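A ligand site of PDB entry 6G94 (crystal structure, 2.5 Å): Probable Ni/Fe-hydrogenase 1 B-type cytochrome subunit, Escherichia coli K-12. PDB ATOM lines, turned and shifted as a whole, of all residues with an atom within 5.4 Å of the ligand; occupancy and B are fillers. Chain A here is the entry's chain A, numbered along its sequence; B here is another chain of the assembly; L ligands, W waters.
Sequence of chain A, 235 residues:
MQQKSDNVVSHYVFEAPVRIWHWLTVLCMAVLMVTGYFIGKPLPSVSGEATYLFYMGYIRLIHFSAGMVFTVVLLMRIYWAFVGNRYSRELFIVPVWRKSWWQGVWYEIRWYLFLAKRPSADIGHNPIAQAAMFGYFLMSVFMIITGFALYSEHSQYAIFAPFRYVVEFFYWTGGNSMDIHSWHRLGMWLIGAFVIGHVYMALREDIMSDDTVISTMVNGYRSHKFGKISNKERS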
ATOM      1  N   MET A  29      15.673 -13.880   2.660  1.00  0.00           N
ATOM      2  CA  MET A  29      16.116 -13.251   1.419  1.00  0.00           C
ATOM      3  C   MET A  29      15.347 -13.766   0.198  1.00  0.00           C
ATOM      4  O   MET A  29      14.818 -12.974  -0.559  1.00  0.00           O
ATOM      5  CB  MET A  29      17.626 -13.477   1.224  1.00  0.00           C
ATOM      6  CG  MET A  29      18.265 -12.594   0.155  1.00  0.00           C
ATOM      7  SD  MET A  29      18.047 -10.869   0.565  1.00  0.00           S
ATOM      8  CE  MET A  29      19.249 -10.655   1.865  1.00  0.00           C
ATOM      9  N   LEU A  32      11.738 -12.436   0.500  1.00  0.00           N
ATOM     10  CA  LEU A  32      11.640 -10.989   0.367  1.00  0.00           C
ATOM     11  C   LEU A  32      11.866 -10.520  -1.068  1.00  0.00           C
ATOM     12  O   LEU A  32      11.351  -9.486  -1.481  1.00  0.00           O
ATOM     13  CB  LEU A  32      12.615 -10.293   1.306  1.00  0.00           C
ATOM     14  CG  LEU A  32      12.195 -10.221   2.766  1.00  0.00           C
ATOM     15  CD1 LEU A  32      13.411 -10.097   3.644  1.00  0.00           C
ATOM     16  CD2 LEU A  32      11.237  -9.064   3.019  1.00  0.00           C
ATOM     17  N   MET A  33      12.636 -11.311  -1.835  1.00  0.00           N
ATOM     18  CA  MET A  33      12.913 -11.038  -3.239  1.00  0.00           C
ATOM     19  C   MET A  33      11.747 -11.461  -4.121  1.00  0.00           C
ATOM     20  O   MET A  33      11.106 -10.624  -4.739  1.00  0.00           O
ATOM     21  CB  MET A  33      14.190 -11.752  -3.686  1.00  0.00           C
ATOM     22  CG  MET A  33      15.472 -11.127  -3.144  1.00  0.00           C
ATOM     23  SD  MET A  33      17.017 -11.677  -3.918  1.00  0.00           S
ATOM     24  CE  MET A  33      16.707 -13.416  -4.243  1.00  0.00           C
ATOM     25  N   GLY A  36       8.695  -9.276  -2.976  1.00  0.00           N
ATOM     26  CA  GLY A  36       8.896  -7.864  -3.269  1.00  0.00           C
ATOM     27  C   GLY A  36       8.898  -7.561  -4.766  1.00  0.00           C
ATOM     28  O   GLY A  36       8.441  -6.501  -5.219  1.00  0.00           O
ATOM     29  N   TYR A  37       9.430  -8.506  -5.547  1.00  0.00           N
ATOM     30  CA  TYR A  37       9.372  -8.429  -6.994  1.00  0.00           C
ATOM     31  C   TYR A  37       7.920  -8.230  -7.480  1.00  0.00           C
ATOM     32  O   TYR A  37       7.659  -7.339  -8.268  1.00  0.00           O
ATOM     33  CB  TYR A  37       9.980  -9.688  -7.646  1.00  0.00           C
ATOM     34  CG  TYR A  37       9.979  -9.608  -9.157  1.00  0.00           C
ATOM     35  CD1 TYR A  37      10.829  -8.718  -9.817  1.00  0.00           C
ATOM     36  CD2 TYR A  37       9.101 -10.395  -9.914  1.00  0.00           C
ATOM     37  CE1 TYR A  37      10.815  -8.621 -11.202  1.00  0.00           C
ATOM     38  CE2 TYR A  37       9.087 -10.297 -11.300  1.00  0.00           C
ATOM     39  CZ  TYR A  37       9.944  -9.407 -11.930  1.00  0.00           C
ATOM     40  OH  TYR A  37       9.951  -9.296 -13.296  1.00  0.00           O
ATOM     41  N   ILE A  39       5.289  -7.292  -5.724  1.00  0.00           N
ATOM     42  CA  ILE A  39       4.618  -6.110  -5.210  1.00  0.00           C
ATOM     43  C   ILE A  39       4.746  -4.980  -6.216  1.00  0.00           C
ATOM     44  O   ILE A  39       3.865  -4.152  -6.330  1.00  0.00           O
ATOM     45  CB  ILE A  39       5.165  -5.714  -3.814  1.00  0.00           C
ATOM     46  CG1 ILE A  39       4.720  -6.748  -2.757  1.00  0.00           C
ATOM     47  CG2 ILE A  39       4.729  -4.303  -3.404  1.00  0.00           C
ATOM     48  CD1 ILE A  39       5.467  -6.714  -1.442  1.00  0.00           C
ATOM     49  N   GLY A  40       5.827  -4.981  -6.988  1.00  0.00           N
ATOM     50  CA  GLY A  40       6.097  -3.924  -7.952  1.00  0.00           C
ATOM     51  C   GLY A  40       5.663  -4.300  -9.357  1.00  0.00           C
ATOM     52  O   GLY A  40       5.104  -3.472 -10.079  1.00  0.00           O
ATOM     53  N   LYS A  41       5.946  -5.532  -9.768  1.00  0.00           N
ATOM     54  CA  LYS A  41       5.431  -6.073 -11.021  1.00  0.00           C
ATOM     55  C   LYS A  41       4.505  -7.244 -10.699  1.00  0.00           C
ATOM     56  O   LYS A  41       4.932  -8.411 -10.715  1.00  0.00           O
ATOM     57  CB  LYS A  41       6.583  -6.510 -11.947  1.00  0.00           C
ATOM     58  CG  LYS A  41       7.418  -5.355 -12.470  1.00  0.00           C
ATOM     59  CD  LYS A  41       6.766  -4.700 -13.693  1.00  0.00           C
ATOM     60  CE  LYS A  41       7.533  -3.451 -14.152  1.00  0.00           C
ATOM     61  NZ  LYS A  41       6.788  -2.652 -15.177  1.00  0.00           N
ATOM     62  N   ARG A  60       1.945  -9.445   0.266  1.00  0.00           N
ATOM     63  CA  ARG A  60       2.404  -8.302   1.041  1.00  0.00           C
ATOM     64  C   ARG A  60       2.613  -8.701   2.485  1.00  0.00           C
ATOM     65  O   ARG A  60       3.486  -8.190   3.152  1.00  0.00           O
ATOM     66  CB  ARG A  60       1.426  -7.126   0.912  1.00  0.00           C
ATOM     67  CG  ARG A  60       1.150  -6.693  -0.520  1.00  0.00           C
ATOM     68  CD  ARG A  60       0.256  -5.471  -0.665  1.00  0.00           C
ATOM     69  NE  ARG A  60       0.525  -4.454   0.352  1.00  0.00           N
ATOM     70  CZ  ARG A  60      -0.340  -4.132   1.288  1.00  0.00           C
ATOM     71  NH1 ARG A  60      -0.046  -3.236   2.202  1.00  0.00           N
ATOM     72  NH2 ARG A  60      -1.502  -4.725   1.300  1.00  0.00           N
ATOM     73  N   HIS A  63       5.626 -10.817   2.831  1.00  0.00           N
ATOM     74  CA  HIS A  63       6.745  -9.897   2.715  1.00  0.00           C
ATOM     75  C   HIS A  63       7.045  -9.160   4.014  1.00  0.00           C
ATOM     76  O   HIS A  63       8.164  -9.199   4.506  1.00  0.00           O
ATOM     77  CB  HIS A  63       6.490  -8.900   1.578  1.00  0.00           C
ATOM     78  CG  HIS A  63       7.711  -8.119   1.184  1.00  0.00           C
ATOM     79  ND1 HIS A  63       8.655  -8.600   0.300  1.00  0.00           N
ATOM     80  CD2 HIS A  63       8.130  -6.880   1.538  1.00  0.00           C
ATOM     81  CE1 HIS A  63       9.605  -7.697   0.148  1.00  0.00           C
ATOM     82  NE2 HIS A  63       9.321  -6.650   0.876  1.00  0.00           N
ATOM     83  N   PHE A  64       6.049  -8.519   4.599  1.00  0.00           N
ATOM     84  CA  PHE A  64       6.297  -7.672   5.777  1.00  0.00           C
ATOM     85  C   PHE A  64       6.833  -8.471   6.964  1.00  0.00           C
ATOM     86  O   PHE A  64       7.641  -7.971   7.762  1.00  0.00           O
ATOM     87  CB  PHE A  64       5.034  -6.918   6.200  1.00  0.00           C
ATOM     88  CG  PHE A  64       4.385  -6.137   5.088  1.00  0.00           C
ATOM     89  CD1 PHE A  64       5.150  -5.647   4.031  1.00  0.00           C
ATOM     90  CD2 PHE A  64       3.025  -5.890   5.108  1.00  0.00           C
ATOM     91  CE1 PHE A  64       4.560  -4.933   3.000  1.00  0.00           C
ATOM     92  CE2 PHE A  64       2.419  -5.179   4.078  1.00  0.00           C
ATOM     93  CZ  PHE A  64       3.191  -4.695   3.022  1.00  0.00           C
ATOM     94  N   GLY A  67      10.203  -9.795   6.429  1.00  0.00           N
ATOM     95  CA  GLY A  67      11.046  -8.659   6.708  1.00  0.00           C
ATOM     96  C   GLY A  67      11.228  -8.419   8.173  1.00  0.00           C
ATOM     97  O   GLY A  67      12.199  -7.798   8.586  1.00  0.00           O
ATOM     98  N   MET A  68      10.283  -8.901   8.985  1.00  0.00           N
ATOM     99  CA  MET A  68      10.394  -8.823  10.435  1.00  0.00           C
ATOM    100  C   MET A  68      11.451  -9.811  10.886  1.00  0.00           C
ATOM    101  O   MET A  68      12.438  -9.413  11.508  1.00  0.00           O
ATOM    102  CB  MET A  68       9.048  -9.122  11.108  1.00  0.00           C
ATOM    103  CG  MET A  68       8.003  -8.024  10.915  1.00  0.00           C
ATOM    104  SD  MET A  68       8.344  -6.572  11.922  1.00  0.00           S
ATOM    105  CE  MET A  68       6.886  -5.572  11.633  1.00  0.00           C
ATOM    106  N   PHE A  70      13.706 -11.518   9.092  1.00  0.00           N
ATOM    107  CA  PHE A  70      14.953 -11.086   8.480  1.00  0.00           C
ATOM    108  C   PHE A  70      15.634 -10.003   9.289  1.00  0.00           C
ATOM    109  O   PHE A  70      16.819 -10.101   9.556  1.00  0.00           O
ATOM    110  CB  PHE A  70      14.721 -10.585   7.056  1.00  0.00           C
ATOM    111  CG  PHE A  70      15.944 -10.003   6.410  1.00  0.00           C
ATOM    112  CD1 PHE A  70      16.890 -10.842   5.817  1.00  0.00           C
ATOM    113  CD2 PHE A  70      16.161  -8.626   6.401  1.00  0.00           C
ATOM    114  CE1 PHE A  70      18.034 -10.320   5.234  1.00  0.00           C
ATOM    115  CE2 PHE A  70      17.298  -8.098   5.816  1.00  0.00           C
ATOM    116  CZ  PHE A  70      18.235  -8.947   5.225  1.00  0.00           C
ATOM    117  N   THR A  71      14.892  -8.968   9.668  1.00  0.00           N
ATOM    118  CA  THR A  71      15.446  -7.832  10.411  1.00  0.00           C
ATOM    119  C   THR A  71      16.035  -8.248  11.766  1.00  0.00           C
ATOM    120  O   THR A  71      17.123  -7.829  12.132  1.00  0.00           O
ATOM    121  CB  THR A  71      14.398  -6.724  10.636  1.00  0.00           C
ATOM    122  OG1 THR A  71      13.951  -6.245   9.371  1.00  0.00           O
ATOM    123  CG2 THR A  71      14.998  -5.552  11.372  1.00  0.00           C
ATOM    124  N   MET A 143      17.950  -1.856   2.935  1.00  0.00           N
ATOM    125  CA  MET A 143      16.684  -2.522   2.649  1.00  0.00           C
ATOM    126  C   MET A 143      15.724  -2.583   3.844  1.00  0.00           C
ATOM    127  O   MET A 143      14.529  -2.868   3.699  1.00  0.00           O
ATOM    128  CB  MET A 143      16.955  -3.926   2.103  1.00  0.00           C
ATOM    129  CG  MET A 143      17.485  -3.901   0.703  1.00  0.00           C
ATOM    130  SD  MET A 143      16.404  -2.908  -0.352  1.00  0.00           S
ATOM    131  CE  MET A 143      15.298  -4.178  -0.940  1.00  0.00           C
ATOM    132  N   ILE A 144      16.266  -2.321   5.038  1.00  0.00           N
ATOM    133  CA  ILE A 144      15.521  -2.353   6.289  1.00  0.00           C
ATOM    134  C   ILE A 144      15.083  -0.945   6.635  1.00  0.00           C
ATOM    135  O   ILE A 144      13.909  -0.722   6.934  1.00  0.00           O
ATOM    136  CB  ILE A 144      16.337  -3.009   7.436  1.00  0.00           C
ATOM    137  CG1 ILE A 144      16.341  -4.544   7.282  1.00  0.00           C
ATOM    138  CG2 ILE A 144      15.801  -2.570   8.803  1.00  0.00           C
ATOM    139  CD1 ILE A 144      17.298  -5.299   8.193  1.00  0.00           C
ATOM    140  N   GLY A 147      12.705  -0.195   3.806  1.00  0.00           N
ATOM    141  CA  GLY A 147      11.567  -1.113   3.899  1.00  0.00           C
ATOM    142  C   GLY A 147      10.613  -0.793   5.044  1.00  0.00           C
ATOM    143  O   GLY A 147       9.399  -0.918   4.884  1.00  0.00           O
ATOM    144  N   PHE A 148      11.170  -0.343   6.181  1.00  0.00           N
ATOM    145  CA  PHE A 148      10.379   0.019   7.357  1.00  0.00           C
ATOM    146  C   PHE A 148       9.792   1.409   7.275  1.00  0.00           C
ATOM    147  O   PHE A 148       8.768   1.685   7.892  1.00  0.00           O
ATOM    148  CB  PHE A 148      11.192  -0.112   8.638  1.00  0.00           C
ATOM    149  CG  PHE A 148      11.052  -1.438   9.297  1.00  0.00           C
ATOM    150  CD1 PHE A 148       9.888  -1.761   9.958  1.00  0.00           C
ATOM    151  CD2 PHE A 148      12.053  -2.382   9.193  1.00  0.00           C
ATOM    152  CE1 PHE A 148       9.720  -2.999  10.539  1.00  0.00           C
ATOM    153  CE2 PHE A 148      11.905  -3.626   9.783  1.00  0.00           C
ATOM    154  CZ  PHE A 148      10.738  -3.936  10.448  1.00  0.00           C
ATOM    155  N   LEU A 150       8.511   2.569   4.677  1.00  0.00           N
ATOM    156  CA  LEU A 150       7.267   2.278   3.995  1.00  0.00           C
ATOM    157  C   LEU A 150       6.210   1.621   4.872  1.00  0.00           C
ATOM    158  O   LEU A 150       5.060   2.009   4.859  1.00  0.00           O
ATOM    159  CB  LEU A 150       7.521   1.386   2.803  1.00  0.00           C
ATOM    160  CG  LEU A 150       8.340   1.969   1.683  1.00  0.00           C
ATOM    161  CD1 LEU A 150       8.584   0.902   0.632  1.00  0.00           C
ATOM    162  CD2 LEU A 150       7.646   3.194   1.122  1.00  0.00           C
ATOM    163  N   TYR A 151       6.617   0.608   5.618  1.00  0.00           N
ATOM    164  CA  TYR A 151       5.730  -0.146   6.493  1.00  0.00           C
ATOM    165  C   TYR A 151       5.135   0.628   7.674  1.00  0.00           C
ATOM    166  O   TYR A 151       3.969   0.480   7.999  1.00  0.00           O
ATOM    167  CB  TYR A 151       6.451  -1.431   6.931  1.00  0.00           C
ATOM    168  CG  TYR A 151       5.636  -2.317   7.815  1.00  0.00           C
ATOM    169  CD1 TYR A 151       5.616  -2.116   9.190  1.00  0.00           C
ATOM    170  CD2 TYR A 151       4.891  -3.367   7.309  1.00  0.00           C
ATOM    171  CE1 TYR A 151       4.862  -2.912  10.026  1.00  0.00           C
ATOM    172  CE2 TYR A 151       4.135  -4.180   8.149  1.00  0.00           C
ATOM    173  CZ  TYR A 151       4.131  -3.948   9.511  1.00  0.00           C
ATOM    174  OH  TYR A 151       3.403  -4.727  10.358  1.00  0.00           O
ATOM    175  N   HIS A 181      10.126   3.675  -2.648  1.00  0.00           N
ATOM    176  CA  HIS A 181       9.761   2.467  -3.370  1.00  0.00           C
ATOM    177  C   HIS A 181      10.758   2.124  -4.436  1.00  0.00           C
ATOM    178  O   HIS A 181      11.027   0.946  -4.693  1.00  0.00           O
ATOM    179  CB  HIS A 181       8.396   2.625  -4.047  1.00  0.00           C
ATOM    180  CG  HIS A 181       7.242   2.206  -3.197  1.00  0.00           C
ATOM    181  ND1 HIS A 181       6.622   0.989  -3.350  1.00  0.00           N
ATOM    182  CD2 HIS A 181       6.618   2.831  -2.164  1.00  0.00           C
ATOM    183  CE1 HIS A 181       5.644   0.891  -2.459  1.00  0.00           C
ATOM    184  NE2 HIS A 181       5.640   1.984  -1.727  1.00  0.00           N
ATOM    185  N   HIS A 184      14.187   1.240  -2.835  1.00  0.00           N
ATOM    186  CA  HIS A 184      13.944  -0.084  -2.252  1.00  0.00           C
ATOM    187  C   HIS A 184      13.983  -1.161  -3.320  1.00  0.00           C
ATOM    188  O   HIS A 184      14.633  -2.188  -3.124  1.00  0.00           O
ATOM    189  CB  HIS A 184      12.602  -0.111  -1.502  1.00  0.00           C
ATOM    190  CG  HIS A 184      12.411  -1.311  -0.604  1.00  0.00           C
ATOM    191  ND1 HIS A 184      13.057  -1.450   0.610  1.00  0.00           N
ATOM    192  CD2 HIS A 184      11.607  -2.395  -0.734  1.00  0.00           C
ATOM    193  CE1 HIS A 184      12.667  -2.574   1.181  1.00  0.00           C
ATOM    194  NE2 HIS A 184      11.779  -3.164   0.394  1.00  0.00           N
ATOM    195  N   ARG A 185      13.316  -0.948  -4.450  1.00  0.00           N
ATOM    196  CA  ARG A 185      13.331  -1.945  -5.522  1.00  0.00           C
ATOM    197  C   ARG A 185      14.725  -2.102  -6.135  1.00  0.00           C
ATOM    198  O   ARG A 185      15.120  -3.201  -6.530  1.00  0.00           O
ATOM    199  CB  ARG A 185      12.305  -1.610  -6.616  1.00  0.00           C
ATOM    200  CG  ARG A 185      12.430  -2.464  -7.870  1.00  0.00           C
ATOM    201  CD  ARG A 185      11.211  -2.422  -8.750  1.00  0.00           C
ATOM    202  NE  ARG A 185      10.356  -3.570  -8.475  1.00  0.00           N
ATOM    203  CZ  ARG A 185      10.183  -4.597  -9.298  1.00  0.00           C
ATOM    204  NH1 ARG A 185       9.403  -5.597  -8.960  1.00  0.00           N
ATOM    205  NH2 ARG A 185      10.818  -4.639 -10.463  1.00  0.00           N
ATOM    206  N   MET A 188      17.022  -4.341  -3.994  1.00  0.00           N
ATOM    207  CA  MET A 188      16.744  -5.723  -4.276  1.00  0.00           C
ATOM    208  C   MET A 188      17.507  -6.278  -5.481  1.00  0.00           C
ATOM    209  O   MET A 188      17.894  -7.423  -5.474  1.00  0.00           O
ATOM    210  CB  MET A 188      15.260  -5.893  -4.483  1.00  0.00           C
ATOM    211  CG  MET A 188      14.819  -7.269  -4.850  1.00  0.00           C
ATOM    212  SD  MET A 188      14.118  -7.252  -6.480  1.00  0.00           S
ATOM    213  CE  MET A 188      13.567  -8.943  -6.554  1.00  0.00           C
ATOM    214  N   ILE A 191      21.412  -6.441  -4.293  1.00  0.00           N
ATOM    215  CA  ILE A 191      21.546  -7.686  -3.530  1.00  0.00           C
ATOM    216  C   ILE A 191      21.622  -8.904  -4.464  1.00  0.00           C
ATOM    217  O   ILE A 191      22.516  -9.739  -4.319  1.00  0.00           O
ATOM    218  CB  ILE A 191      20.411  -7.804  -2.493  1.00  0.00           C
ATOM    219  CG1 ILE A 191      20.743  -6.928  -1.276  1.00  0.00           C
ATOM    220  CG2 ILE A 191      20.146  -9.259  -2.084  1.00  0.00           C
ATOM    221  CD1 ILE A 191      19.526  -6.565  -0.474  1.00  0.00           C
ATOM    222  N   PHE B 196      -7.355  -4.432  -5.163  1.00  0.00           N
ATOM    223  CA  PHE B 196      -5.906  -4.376  -5.003  1.00  0.00           C
ATOM    224  C   PHE B 196      -5.392  -5.563  -4.208  1.00  0.00           C
ATOM    225  O   PHE B 196      -4.556  -6.300  -4.696  1.00  0.00           O
ATOM    226  CB  PHE B 196      -5.470  -3.069  -4.331  1.00  0.00           C
ATOM    227  CG  PHE B 196      -4.014  -3.019  -3.982  1.00  0.00           C
ATOM    228  CD1 PHE B 196      -3.074  -2.658  -4.940  1.00  0.00           C
ATOM    229  CD2 PHE B 196      -3.569  -3.278  -2.694  1.00  0.00           C
ATOM    230  CE1 PHE B 196      -1.721  -2.580  -4.628  1.00  0.00           C
ATOM    231  CE2 PHE B 196      -2.227  -3.198  -2.376  1.00  0.00           C
ATOM    232  CZ  PHE B 196      -1.297  -2.850  -3.346  1.00  0.00           C
ATOM    233  N   TYR B 217      -3.628  -0.240 -10.220  1.00  0.00           N
ATOM    234  CA  TYR B 217      -2.252  -0.268  -9.753  1.00  0.00           C
ATOM    235  C   TYR B 217      -1.300  -0.580 -10.921  1.00  0.00           C
ATOM    236  O   TYR B 217      -0.270   0.074 -11.074  1.00  0.00           O
ATOM    237  CB  TYR B 217      -2.147  -1.282  -8.615  1.00  0.00           C
ATOM    238  CG  TYR B 217      -0.819  -1.458  -7.905  1.00  0.00           C
ATOM    239  CD1 TYR B 217      -0.247  -0.428  -7.175  1.00  0.00           C
ATOM    240  CD2 TYR B 217      -0.197  -2.694  -7.858  1.00  0.00           C
ATOM    241  CE1 TYR B 217       0.935  -0.589  -6.472  1.00  0.00           C
ATOM    242  CE2 TYR B 217       0.983  -2.871  -7.152  1.00  0.00           C
ATOM    243  CZ  TYR B 217       1.543  -1.817  -6.455  1.00  0.00           C
ATOM    244  OH  TYR B 217       2.715  -1.958  -5.750  1.00  0.00           O
ATOM    245  N   PRO B 224      -0.742   4.770  -3.886  1.00  0.00           N
ATOM    246  CA  PRO B 224       0.028   4.266  -2.725  1.00  0.00           C
ATOM    247  C   PRO B 224       1.059   5.219  -2.125  1.00  0.00           C
ATOM    248  O   PRO B 224       1.488   5.012  -0.988  1.00  0.00           O
ATOM    249  CB  PRO B 224       0.707   3.021  -3.276  1.00  0.00           C
ATOM    250  CG  PRO B 224      -0.263   2.526  -4.296  1.00  0.00           C
ATOM    251  CD  PRO B 224      -0.874   3.721  -4.922  1.00  0.00           C
ATOM    252  N   VAL B 267       7.225   0.848 -11.962  1.00  0.00           N
ATOM    253  CA  VAL B 267       8.634   1.148 -11.692  1.00  0.00           C
ATOM    254  C   VAL B 267       8.979   2.412 -12.491  1.00  0.00           C
ATOM    255  O   VAL B 267       8.792   2.458 -13.717  1.00  0.00           O
ATOM    256  CB  VAL B 267       9.519  -0.049 -12.082  1.00  0.00           C
ATOM    257  CG1 VAL B 267      10.966   0.203 -11.684  1.00  0.00           C
ATOM    258  CG2 VAL B 267       8.973  -1.333 -11.427  1.00  0.00           C
HETATM  259  C1  LIG L   1       8.253  -3.687  -1.138  1.00  0.00           C
HETATM  260  C2  LIG L   1      12.098  -6.461  -1.675  1.00  0.00           C
HETATM  261  C3  LIG L   1      13.182  -5.844   2.969  1.00  0.00           C
HETATM  262  C4  LIG L   1       8.995  -3.580   3.604  1.00  0.00           C
HETATM  263  C5  LIG L   1       9.284  -4.397  -1.671  1.00  0.00           C
HETATM  264  C6  LIG L   1       9.556  -4.431  -3.042  1.00  0.00           C
HETATM  265  C7  LIG L   1      10.641  -5.202  -3.205  1.00  0.00           C
HETATM  266  C8  LIG L   1      11.033  -5.650  -1.934  1.00  0.00           C
HETATM  267  C9  LIG L   1      11.282  -5.526  -4.530  1.00  0.00           C
HETATM  268  C10 LIG L   1       8.748  -3.753  -4.136  1.00  0.00           C
HETATM  269  C11 LIG L   1       9.118  -2.291  -4.326  1.00  0.00           C
HETATM  270  C12 LIG L   1       8.291  -1.713  -5.427  1.00  0.00           C
HETATM  271  O1  LIG L   1       8.404  -2.038  -6.612  1.00  0.00           O
HETATM  272  O2  LIG L   1       7.461  -0.849  -5.141  1.00  0.00           O
HETATM  273  C13 LIG L   1      12.748  -6.510  -0.430  1.00  0.00           C
HETATM  274  C14 LIG L   1      13.995  -7.171  -0.229  1.00  0.00           C
HETATM  275  C15 LIG L   1      14.295  -6.975   1.075  1.00  0.00           C
HETATM  276  C16 LIG L   1      13.199  -6.207   1.644  1.00  0.00           C
HETATM  277  C17 LIG L   1      14.800  -7.914  -1.268  1.00  0.00           C
HETATM  278  C18 LIG L   1      15.460  -7.414   1.855  1.00  0.00           C
HETATM  279  C19 LIG L   1      16.328  -8.284   1.376  1.00  0.00           C
HETATM  280  C20 LIG L   1      12.098  -5.227   3.565  1.00  0.00           C
HETATM  281  C21 LIG L   1      11.951  -5.015   4.942  1.00  0.00           C
HETATM  282  C22 LIG L   1      10.763  -4.361   5.114  1.00  0.00           C
HETATM  283  C23 LIG L   1      10.190  -4.186   3.835  1.00  0.00           C
HETATM  284  C24 LIG L   1      12.920  -5.386   6.035  1.00  0.00           C
HETATM  285  C25 LIG L   1      10.216  -3.935   6.418  1.00  0.00           C
HETATM  286  C26 LIG L   1       9.039  -4.384   6.826  1.00  0.00           C
HETATM  287  C27 LIG L   1       8.504  -3.402   2.327  1.00  0.00           C
HETATM  288  C28 LIG L   1       7.295  -2.623   2.115  1.00  0.00           C
HETATM  289  C29 LIG L   1       7.063  -2.656   0.776  1.00  0.00           C
HETATM  290  C30 LIG L   1       8.165  -3.447   0.212  1.00  0.00           C
HETATM  291  C31 LIG L   1       6.489  -1.974   3.211  1.00  0.00           C
HETATM  292  C32 LIG L   1       5.946  -2.015  -0.034  1.00  0.00           C
HETATM  293  C33 LIG L   1       4.559  -2.419   0.467  1.00  0.00           C
HETATM  294  C34 LIG L   1       3.413  -1.889  -0.347  1.00  0.00           C
HETATM  295  O3  LIG L   1       3.070  -0.693  -0.292  1.00  0.00           O
HETATM  296  O4  LIG L   1       2.772  -2.645  -1.084  1.00  0.00           O
HETATM  297  N1  LIG L   1      10.210  -5.123  -0.992  1.00  0.00           N
HETATM  298  N2  LIG L   1      12.317  -5.963   0.698  1.00  0.00           N
HETATM  299  N3  LIG L   1      11.002  -4.764   2.926  1.00  0.00           N
HETATM  300  N4  LIG L   1       8.999  -3.866   1.175  1.00  0.00           N
HETATM  301 FE1  LIG L   1      10.532  -4.868   0.930  1.00  0.00          FE
HETATM  302  O   HOH W   1      -0.160  -1.092  -0.605  1.00  0.00           O
HETATM  303  O   HOH W   2       2.067  -1.044   2.947  1.00  0.00           O
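O4 of the ligand is in salt-bridge range of NE of Arg 60 (3.2 Å).
ND1 of His 181 lies within hydrogen-bond range of O2 of the ligand, at 2.7 Å.
A ring nitrogen (NE2) of His 63 binds an iron atom (FE1) of the ligand, 2.2 Å away.
The guanidinium group (NE) of Arg 185 is in salt-bridge range of an oxygen (O1) of the ligand (3.1 Å).
A ring nitrogen (NE2) of His 184 binds an iron atom (FE1) of the ligand (2.2 Å).
The backbone carbonyl oxygen (O) of Leu 32 lies close to a ring nitrogen (ND1) of His 63 (3.4 Å).
A ring nitrogen (ND1) of His 184 lies within hydrogen-bond range of the side-chain sulfur (SD) of Met 143 (3.8 Å).
The guanidinium group (NH1) of Arg 185 is in hydrogen-bond range of the backbone carbonyl oxygen (O) of Tyr 37, 2.6 Å away.
ND1 of His 63 is in hydrogen-bond range of N of Gly 36.
The backbone carbonyl oxygen (O) of Gly 67 lies within hydrogen-bond range of the side-chain hydroxyl (OG1) of Thr 71, 2.5 Å away.
The backbone NH (N) of Gly 147 sits at hydrogen-bond distance from a ring nitrogen (ND1) of His 184 (3.5 Å).
The side-chain hydroxyl of Tyr 217 of chain B is in hydrogen-bond range of the backbone carbonyl oxygen of Ile 39 (2.5 Å).
Residues that only touch the ligand: Met 29 (3.2 Å), Leu 32 (3.1 Å), Met 33 (3.8 Å), Gly 36 (3.0 Å), Tyr 37 (3.7 Å), Ile 39 (3.5 Å), Gly 40 (3.3 Å), Phe 64 (3.5 Å), Gly 67 (3.6 Å), Thr 71 (3.6 Å), Met 143 (3.3 Å), Ile 144 (3.7 Å), Gly 147 (3.0 Å), Phe 148 (3.7 Å), Leu 150 (3.5 Å), Tyr 151 (3.5 Å) and Met 188 (3.6 Å).
Of the 30 residues printed, 22 come within 4 Å of the ligand.
The nearest printed residue that does not touch the ligand is Ile 191 (4.1 Å).
Water W2 bridges the guanidinium group of Arg 60 and an oxygen (O3) of the ligand.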
